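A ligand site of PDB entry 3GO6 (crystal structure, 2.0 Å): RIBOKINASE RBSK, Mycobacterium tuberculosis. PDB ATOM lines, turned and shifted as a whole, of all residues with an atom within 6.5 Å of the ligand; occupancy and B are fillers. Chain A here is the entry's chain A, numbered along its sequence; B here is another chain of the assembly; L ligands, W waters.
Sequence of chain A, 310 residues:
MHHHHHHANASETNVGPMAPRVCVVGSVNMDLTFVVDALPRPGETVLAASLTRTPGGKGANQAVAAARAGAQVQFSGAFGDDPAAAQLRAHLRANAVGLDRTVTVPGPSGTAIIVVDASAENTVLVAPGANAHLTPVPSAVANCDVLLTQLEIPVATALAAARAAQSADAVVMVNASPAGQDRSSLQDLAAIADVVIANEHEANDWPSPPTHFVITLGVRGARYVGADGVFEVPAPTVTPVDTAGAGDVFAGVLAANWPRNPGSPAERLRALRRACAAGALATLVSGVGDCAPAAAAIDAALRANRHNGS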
ATOM      1  N   SER A  27      15.770 -12.874   9.769  1.00  0.00           N
ATOM      2  CA  SER A  27      15.844 -11.983  10.912  1.00  0.00           C
ATOM      3  C   SER A  27      15.508 -12.657  12.232  1.00  0.00           C
ATOM      4  O   SER A  27      14.794 -13.654  12.295  1.00  0.00           O
ATOM      5  CB  SER A  27      14.874 -10.833  10.689  1.00  0.00           C
ATOM      6  OG  SER A  27      13.614 -11.383  10.414  1.00  0.00           O
ATOM      7  N   VAL A  28      16.044 -12.076  13.292  1.00  0.00           N
ATOM      8  CA  VAL A  28      15.775 -12.528  14.658  1.00  0.00           C
ATOM      9  C   VAL A  28      15.603 -11.280  15.514  1.00  0.00           C
ATOM     10  O   VAL A  28      16.443 -10.389  15.516  1.00  0.00           O
ATOM     11  CB  VAL A  28      16.894 -13.520  15.191  1.00  0.00           C
ATOM     12  CG1 VAL A  28      18.327 -12.896  15.088  1.00  0.00           C
ATOM     13  CG2 VAL A  28      16.564 -14.029  16.627  1.00  0.00           C
ATOM     14  N   ASN A  29      14.462 -11.203  16.220  1.00  0.00           N
ATOM     15  CA  ASN A  29      14.051  -9.998  16.949  1.00  0.00           C
ATOM     16  C   ASN A  29      13.598 -10.433  18.318  1.00  0.00           C
ATOM     17  O   ASN A  29      13.071 -11.533  18.457  1.00  0.00           O
ATOM     18  CB  ASN A  29      12.816  -9.330  16.289  1.00  0.00           C
ATOM     19  CG  ASN A  29      13.055  -8.896  14.850  1.00  0.00           C
ATOM     20  OD1 ASN A  29      14.102  -8.357  14.525  1.00  0.00           O
ATOM     21  ND2 ASN A  29      12.071  -9.153  13.973  1.00  0.00           N
ATOM     22  N   MET A  30      13.742  -9.576  19.322  1.00  0.00           N
ATOM     23  CA  MET A  30      12.958  -9.754  20.552  1.00  0.00           C
ATOM     24  C   MET A  30      11.557  -9.123  20.356  1.00  0.00           C
ATOM     25  O   MET A  30      11.460  -7.981  19.911  1.00  0.00           O
ATOM     26  CB  MET A  30      13.682  -9.121  21.747  1.00  0.00           C
ATOM     27  CG  MET A  30      13.005  -9.412  23.082  1.00  0.00           C
ATOM     28  SD  MET A  30      13.180 -11.138  23.606  1.00  0.00           S
ATOM     29  CE  MET A  30      14.979 -11.311  23.784  1.00  0.00           C
ATOM     30  N   ASP A  31      10.506  -9.877  20.676  1.00  0.00           N
ATOM     31  CA  ASP A  31       9.124  -9.485  20.429  1.00  0.00           C
ATOM     32  C   ASP A  31       8.483  -8.987  21.699  1.00  0.00           C
ATOM     33  O   ASP A  31       8.562  -9.649  22.746  1.00  0.00           O
ATOM     34  CB  ASP A  31       8.293 -10.689  19.949  1.00  0.00           C
ATOM     35  CG  ASP A  31       8.588 -11.097  18.507  1.00  0.00           C
ATOM     36  OD1 ASP A  31       9.268 -10.333  17.796  1.00  0.00           O
ATOM     37  OD2 ASP A  31       8.138 -12.191  18.098  1.00  0.00           O
ATOM     38  N   PRO A  55      11.493 -14.175  22.500  1.00  0.00           N
ATOM     39  CA  PRO A  55      12.273 -14.254  21.252  1.00  0.00           C
ATOM     40  C   PRO A  55      11.396 -14.546  20.039  1.00  0.00           C
ATOM     41  O   PRO A  55      10.450 -15.360  20.122  1.00  0.00           O
ATOM     42  CB  PRO A  55      13.193 -15.452  21.485  1.00  0.00           C
ATOM     43  CG  PRO A  55      13.296 -15.589  22.943  1.00  0.00           C
ATOM     44  CD  PRO A  55      11.948 -15.173  23.498  1.00  0.00           C
ATOM     45  N   GLY A  56      11.688 -13.869  18.937  1.00  0.00           N
ATOM     46  CA  GLY A  56      11.011 -14.156  17.666  1.00  0.00           C
ATOM     47  C   GLY A  56      11.803 -13.638  16.491  1.00  0.00           C
ATOM     48  O   GLY A  56      13.029 -13.792  16.456  1.00  0.00           O
ATOM     49  N   GLY A  57      11.126 -12.985  15.557  1.00  0.00           N
ATOM     50  CA  GLY A  57      11.714 -12.610  14.270  1.00  0.00           C
ATOM     51  C   GLY A  57      11.270 -13.588  13.202  1.00  0.00           C
ATOM     52  O   GLY A  57      11.294 -14.798  13.427  1.00  0.00           O
ATOM     53  N   LYS A  58      10.860 -13.082  12.044  1.00  0.00           N
ATOM     54  CA  LYS A  58      10.422 -13.969  10.941  1.00  0.00           C
ATOM     55  C   LYS A  58      11.393 -15.113  10.660  1.00  0.00           C
ATOM     56  O   LYS A  58      10.978 -16.254  10.452  1.00  0.00           O
ATOM     57  CB  LYS A  58      10.225 -13.181   9.634  1.00  0.00           C
ATOM     58  CG  LYS A  58       8.981 -12.334   9.620  1.00  0.00           C
ATOM     59  CD  LYS A  58       8.803 -11.684   8.230  1.00  0.00           C
ATOM     60  CE  LYS A  58       7.766 -10.571   8.293  1.00  0.00           C
ATOM     61  NZ  LYS A  58       6.550 -10.926   9.140  1.00  0.00           N
ATOM     62  N   GLY A  59      12.686 -14.837  10.610  1.00  0.00           N
ATOM     63  CA  GLY A  59      13.648 -15.871  10.235  1.00  0.00           C
ATOM     64  C   GLY A  59      13.756 -16.918  11.334  1.00  0.00           C
ATOM     65  O   GLY A  59      13.690 -18.136  11.081  1.00  0.00           O
ATOM     66  N   ASN A  61      11.555 -17.556  13.681  1.00  0.00           N
ATOM     67  CA  ASN A  61      10.264 -18.259  13.776  1.00  0.00           C
ATOM     68  C   ASN A  61      10.136 -19.325  12.688  1.00  0.00           C
ATOM     69  O   ASN A  61       9.623 -20.426  12.944  1.00  0.00           O
ATOM     70  CB  ASN A  61       9.076 -17.290  13.607  1.00  0.00           C
ATOM     71  CG  ASN A  61       8.958 -16.290  14.729  1.00  0.00           C
ATOM     72  OD1 ASN A  61       9.573 -16.438  15.782  1.00  0.00           O
ATOM     73  ND2 ASN A  61       8.130 -15.259  14.518  1.00  0.00           N
ATOM     74  N   GLN A  62      10.556 -18.990  11.473  1.00  0.00           N
ATOM     75  CA  GLN A  62      10.467 -19.939  10.352  1.00  0.00           C
ATOM     76  C   GLN A  62      11.435 -21.113  10.535  1.00  0.00           C
ATOM     77  O   GLN A  62      11.086 -22.257  10.239  1.00  0.00           O
ATOM     78  CB  GLN A  62      10.663 -19.234   9.014  1.00  0.00           C
ATOM     79  CG  GLN A  62       9.464 -18.309   8.735  1.00  0.00           C
ATOM     80  CD  GLN A  62       9.592 -17.471   7.504  1.00  0.00           C
ATOM     81  OE1 GLN A  62      10.423 -17.709   6.656  1.00  0.00           O
ATOM     82  NE2 GLN A  62       8.720 -16.456   7.409  1.00  0.00           N
ATOM     83  N   THR A 111      14.054  -5.441  17.365  1.00  0.00           N
ATOM     84  CA  THR A 111      12.925  -5.373  18.302  1.00  0.00           C
ATOM     85  C   THR A 111      11.657  -5.353  17.467  1.00  0.00           C
ATOM     86  O   THR A 111      11.578  -4.596  16.492  1.00  0.00           O
ATOM     87  CB  THR A 111      12.943  -4.051  19.163  1.00  0.00           C
ATOM     88  OG1 THR A 111      14.169  -3.969  19.919  1.00  0.00           O
ATOM     89  CG2 THR A 111      11.736  -4.008  20.146  1.00  0.00           C
ATOM     90  N   ALA A 112      10.666  -6.170  17.828  1.00  0.00           N
ATOM     91  CA  ALA A 112       9.375  -6.055  17.156  1.00  0.00           C
ATOM     92  C   ALA A 112       8.215  -5.838  18.116  1.00  0.00           C
ATOM     93  O   ALA A 112       8.250  -6.348  19.237  1.00  0.00           O
ATOM     94  CB  ALA A 112       9.107  -7.280  16.306  1.00  0.00           C
ATOM     95  N   ILE A 113       7.205  -5.089  17.667  1.00  0.00           N
ATOM     96  CA  ILE A 113       5.990  -4.874  18.450  1.00  0.00           C
ATOM     97  C   ILE A 113       4.874  -5.632  17.748  1.00  0.00           C
ATOM     98  O   ILE A 113       4.588  -5.403  16.572  1.00  0.00           O
ATOM     99  CB  ILE A 113       5.579  -3.362  18.515  1.00  0.00           C
ATOM    100  CG1 ILE A 113       6.734  -2.469  18.979  1.00  0.00           C
ATOM    101  CG2 ILE A 113       4.312  -3.164  19.403  1.00  0.00           C
ATOM    102  CD1 ILE A 113       7.343  -2.898  20.323  1.00  0.00           C
ATOM    103  N   ILE A 114       4.239  -6.550  18.480  1.00  0.00           N
ATOM    104  CA  ILE A 114       3.110  -7.304  17.957  1.00  0.00           C
ATOM    105  C   ILE A 114       1.892  -6.871  18.766  1.00  0.00           C
ATOM    106  O   ILE A 114       1.906  -6.922  19.997  1.00  0.00           O
ATOM    107  CB  ILE A 114       3.294  -8.831  18.123  1.00  0.00           C
ATOM    108  CG1 ILE A 114       4.739  -9.311  17.813  1.00  0.00           C
ATOM    109  CG2 ILE A 114       2.147  -9.610  17.400  1.00  0.00           C
ATOM    110  CD1 ILE A 114       5.116  -9.234  16.469  1.00  0.00           C
ATOM    111  N   ASN A 122      -3.731  -9.352  14.089  1.00  0.00           N
ATOM    112  CA  ASN A 122      -2.464  -8.822  14.632  1.00  0.00           C
ATOM    113  C   ASN A 122      -1.836  -7.807  13.687  1.00  0.00           C
ATOM    114  O   ASN A 122      -2.102  -7.831  12.476  1.00  0.00           O
ATOM    115  CB  ASN A 122      -1.486  -9.974  14.919  1.00  0.00           C
ATOM    116  CG  ASN A 122      -0.804 -10.522  13.649  1.00  0.00           C
ATOM    117  OD1 ASN A 122       0.257 -10.025  13.250  1.00  0.00           O
ATOM    118  ND2 ASN A 122      -1.398 -11.536  13.026  1.00  0.00           N
ATOM    119  N   VAL A 124       2.222  -6.022  13.069  1.00  0.00           N
ATOM    120  CA  VAL A 124       3.635  -6.208  13.448  1.00  0.00           C
ATOM    121  C   VAL A 124       4.432  -4.984  13.001  1.00  0.00           C
ATOM    122  O   VAL A 124       4.306  -4.549  11.835  1.00  0.00           O
ATOM    123  CB  VAL A 124       4.213  -7.509  12.816  1.00  0.00           C
ATOM    124  CG1 VAL A 124       5.748  -7.638  13.059  1.00  0.00           C
ATOM    125  CG2 VAL A 124       3.497  -8.742  13.354  1.00  0.00           C
ATOM    126  N   LEU A 125       5.232  -4.426  13.918  1.00  0.00           N
ATOM    127  CA  LEU A 125       6.110  -3.307  13.628  1.00  0.00           C
ATOM    128  C   LEU A 125       7.515  -3.683  14.073  1.00  0.00           C
ATOM    129  O   LEU A 125       7.718  -4.059  15.236  1.00  0.00           O
ATOM    130  CB  LEU A 125       5.659  -2.070  14.425  1.00  0.00           C
ATOM    131  CG  LEU A 125       6.546  -0.835  14.404  1.00  0.00           C
ATOM    132  CD1 LEU A 125       6.668  -0.274  13.012  1.00  0.00           C
ATOM    133  CD2 LEU A 125       6.034   0.250  15.377  1.00  0.00           C
ATOM    134  N   VAL A 126       8.495  -3.514  13.181  1.00  0.00           N
ATOM    135  CA  VAL A 126       9.848  -4.056  13.430  1.00  0.00           C
ATOM    136  C   VAL A 126      10.883  -2.944  13.316  1.00  0.00           C
ATOM    137  O   VAL A 126      10.920  -2.220  12.323  1.00  0.00           O
ATOM    138  CB  VAL A 126      10.238  -5.161  12.404  1.00  0.00           C
ATOM    139  CG1 VAL A 126      11.647  -5.696  12.684  1.00  0.00           C
ATOM    140  CG2 VAL A 126       9.197  -6.304  12.413  1.00  0.00           C
ATOM    141  N   GLU A 152      13.192  -8.763   6.024  1.00  0.00           N
ATOM    142  CA  GLU A 152      13.580  -7.810   7.088  1.00  0.00           C
ATOM    143  C   GLU A 152      15.092  -7.557   7.079  1.00  0.00           C
ATOM    144  O   GLU A 152      15.559  -6.499   7.521  1.00  0.00           O
ATOM    145  CB  GLU A 152      13.148  -8.289   8.489  1.00  0.00           C
ATOM    146  CG  GLU A 152      11.626  -8.546   8.632  1.00  0.00           C
ATOM    147  CD  GLU A 152      11.241  -8.946  10.074  1.00  0.00           C
ATOM    148  OE1 GLU A 152      12.152  -9.210  10.916  1.00  0.00           O
ATOM    149  OE2 GLU A 152      10.037  -8.966  10.384  1.00  0.00           O
ATOM    150  N   ALA A 244      -0.958 -14.091  15.181  1.00  0.00           N
ATOM    151  CA  ALA A 244       0.444 -13.677  15.050  1.00  0.00           C
ATOM    152  C   ALA A 244       1.353 -14.902  15.063  1.00  0.00           C
ATOM    153  O   ALA A 244       1.139 -15.854  15.836  1.00  0.00           O
ATOM    154  CB  ALA A 244       0.816 -12.709  16.159  1.00  0.00           C
ATOM    155  N   GLY A 245       2.325 -14.903  14.158  1.00  0.00           N
ATOM    156  CA  GLY A 245       3.267 -15.989  14.082  1.00  0.00           C
ATOM    157  C   GLY A 245       2.808 -17.119  13.185  1.00  0.00           C
ATOM    158  O   GLY A 245       3.604 -17.957  12.809  1.00  0.00           O
ATOM    159  N   ALA A 246       1.518 -17.176  12.829  1.00  0.00           N
ATOM    160  CA  ALA A 246       1.038 -18.339  12.068  1.00  0.00           C
ATOM    161  C   ALA A 246       1.602 -18.385  10.656  1.00  0.00           C
ATOM    162  O   ALA A 246       1.840 -19.489  10.107  1.00  0.00           O
ATOM    163  CB  ALA A 246      -0.477 -18.408  12.061  1.00  0.00           C
ATOM    164  N   GLY A 247       1.775 -17.213  10.053  1.00  0.00           N
ATOM    165  CA  GLY A 247       2.368 -17.129   8.717  1.00  0.00           C
ATOM    166  C   GLY A 247       3.799 -17.664   8.683  1.00  0.00           C
ATOM    167  O   GLY A 247       4.195 -18.321   7.724  1.00  0.00           O
ATOM    168  N   ASP A 248       4.579 -17.386   9.732  1.00  0.00           N
ATOM    169  CA  ASP A 248       5.955 -17.925   9.837  1.00  0.00           C
ATOM    170  C   ASP A 248       5.923 -19.424   9.986  1.00  0.00           C
ATOM    171  O   ASP A 248       6.778 -20.115   9.453  1.00  0.00           O
ATOM    172  CB  ASP A 248       6.684 -17.302  11.030  1.00  0.00           C
ATOM    173  CG  ASP A 248       6.958 -15.826  10.830  1.00  0.00           C
ATOM    174  OD1 ASP A 248       7.103 -15.401   9.652  1.00  0.00           O
ATOM    175  OD2 ASP A 248       6.992 -15.090  11.846  1.00  0.00           O
ATOM    176  N   VAL A 288       3.944 -15.777  19.634  1.00  0.00           N
ATOM    177  CA  VAL A 288       4.351 -15.607  18.249  1.00  0.00           C
ATOM    178  C   VAL A 288       5.469 -16.613  17.955  1.00  0.00           C
ATOM    179  O   VAL A 288       5.356 -17.431  17.031  1.00  0.00           O
ATOM    180  CB  VAL A 288       4.813 -14.137  18.007  1.00  0.00           C
ATOM    181  CG1 VAL A 288       5.290 -13.925  16.581  1.00  0.00           C
ATOM    182  CG2 VAL A 288       3.675 -13.162  18.342  1.00  0.00           C
ATOM    183  N   GLY A 289       6.526 -16.552  18.759  1.00  0.00           N
ATOM    184  CA  GLY A 289       7.730 -17.344  18.490  1.00  0.00           C
ATOM    185  C   GLY A 289       7.688 -18.794  18.958  1.00  0.00           C
ATOM    186  O   GLY A 289       8.553 -19.594  18.603  1.00  0.00           O
ATOM    187  N   THR B  45       3.111  -6.365   8.216  1.00  0.00           N
ATOM    188  CA  THR B  45       4.385  -6.067   8.878  1.00  0.00           C
ATOM    189  C   THR B  45       4.977  -4.820   8.244  1.00  0.00           C
ATOM    190  O   THR B  45       5.143  -4.756   7.019  1.00  0.00           O
ATOM    191  CB  THR B  45       5.380  -7.226   8.700  1.00  0.00           C
ATOM    192  OG1 THR B  45       4.818  -8.417   9.260  1.00  0.00           O
ATOM    193  CG2 THR B  45       6.738  -6.910   9.399  1.00  0.00           C
HETATM  194  O1  LIG L   1       5.698 -12.909  11.737  1.00  0.00           O
HETATM  195  C1  LIG L   1       5.824 -12.421  13.088  1.00  0.00           C
HETATM  196  C2  LIG L   1       7.265 -11.931  13.303  1.00  0.00           C
HETATM  197  O2  LIG L   1       7.452 -10.725  12.543  1.00  0.00           O
HETATM  198  C3  LIG L   1       7.556 -11.525  14.742  1.00  0.00           C
HETATM  199  O3  LIG L   1       8.224 -12.541  15.530  1.00  0.00           O
HETATM  200  C4  LIG L   1       8.376 -10.248  14.611  1.00  0.00           C
HETATM  201  O4  LIG L   1       9.674 -10.381  15.193  1.00  0.00           O
HETATM  202  C5  LIG L   1       8.445  -9.893  13.137  1.00  0.00           C
HETATM  203  O5  LIG L   1       9.705 -10.242  12.560  1.00  0.00           O
HETATM  204  O   HOH W   1       2.444 -12.386  12.747  1.00  0.00           O
HETATM  205  O   HOH W   2       3.830 -14.834  11.295  1.00  0.00           O
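The side-chain amino group (NZ) of Lys 58 lies within hydrogen-bond range of an oxygen (O1) of the ligand, 3.4 Å away. O3 of the ligand sits at hydrogen-bond distance from OD2 of Asp 31. An oxygen (O5) of the ligand lies within hydrogen-bond range of the backbone NH (N) of Lys 58 (3.1 Å). An oxygen (O1) of the ligand is in hydrogen-bond range of the side-chain carboxylate (OD2) of Asp 248. An oxygen (O3) of the ligand sits at hydrogen-bond distance from the backbone NH (N) of Gly 57 (2.9 Å). An oxygen (O4) of the ligand sits at hydrogen-bond distance from the side-chain amide nitrogen (ND2) of Asn 29, at 3.0 Å. The side-chain carboxylate (OE2) of Glu 152 sits at hydrogen-bond distance from an oxygen (O5) of the ligand (2.5 Å). O3 of the ligand is in hydrogen-bond range of ND2 of Asn 61, 2.9 Å away.
The side-chain carboxylate of Asp 248 sits at hydrogen-bond distance from the side-chain amide nitrogen of Gln 62 (3.0 Å). OD2 of Asp 248 lies within hydrogen-bond range of ND2 of Asn 61 (2.9 Å). The side-chain carboxylate (OE1) of Glu 152 is in hydrogen-bond range of the side-chain amide nitrogen (ND2) of Asn 29 (3.1 Å). The side-chain amino group of Lys 58 sits at hydrogen-bond distance from the side-chain hydroxyl of Thr 45 of chain B (3.1 Å). N of Gly 56 lies within hydrogen-bond range of O of Asn 29, at 2.8 Å. The backbone carbonyl oxygen (O) of Gly 57 lies close to the side-chain amide oxygen (OD1) of Asn 61, at 3.3 Å. OE1 of Glu 152 sits at hydrogen-bond distance from OG of Ser 27. N of Ala 112 lies within hydrogen-bond range of O of Met 30 (2.9 Å).
Gly 56 touches the ligand. Ala 112 touches the ligand (CB to O4, 3.3 Å). CD1 of Ile 114 touches C3 of the ligand, 3.8 Å away. CG1 of Val 124 touches C5 of the ligand, 3.5 Å away. Val 126 touches the ligand (CG2 to C5, 3.7 Å). CG1 of Val 288 touches O3 of the ligand, at 3.4 Å. Hydrophobic or aromatic side chains that line the ligand: Ala 112, Ile 114, Val 124, Val 126 and Val 288.
Water W1 lies within hydrogen-bond range of the backbone NH (N) of Gly 245 (2.9 Å), the side-chain amide oxygen (OD1) of Asn 122 (3.3 Å) and an oxygen (O1) of the ligand (3.4 Å).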
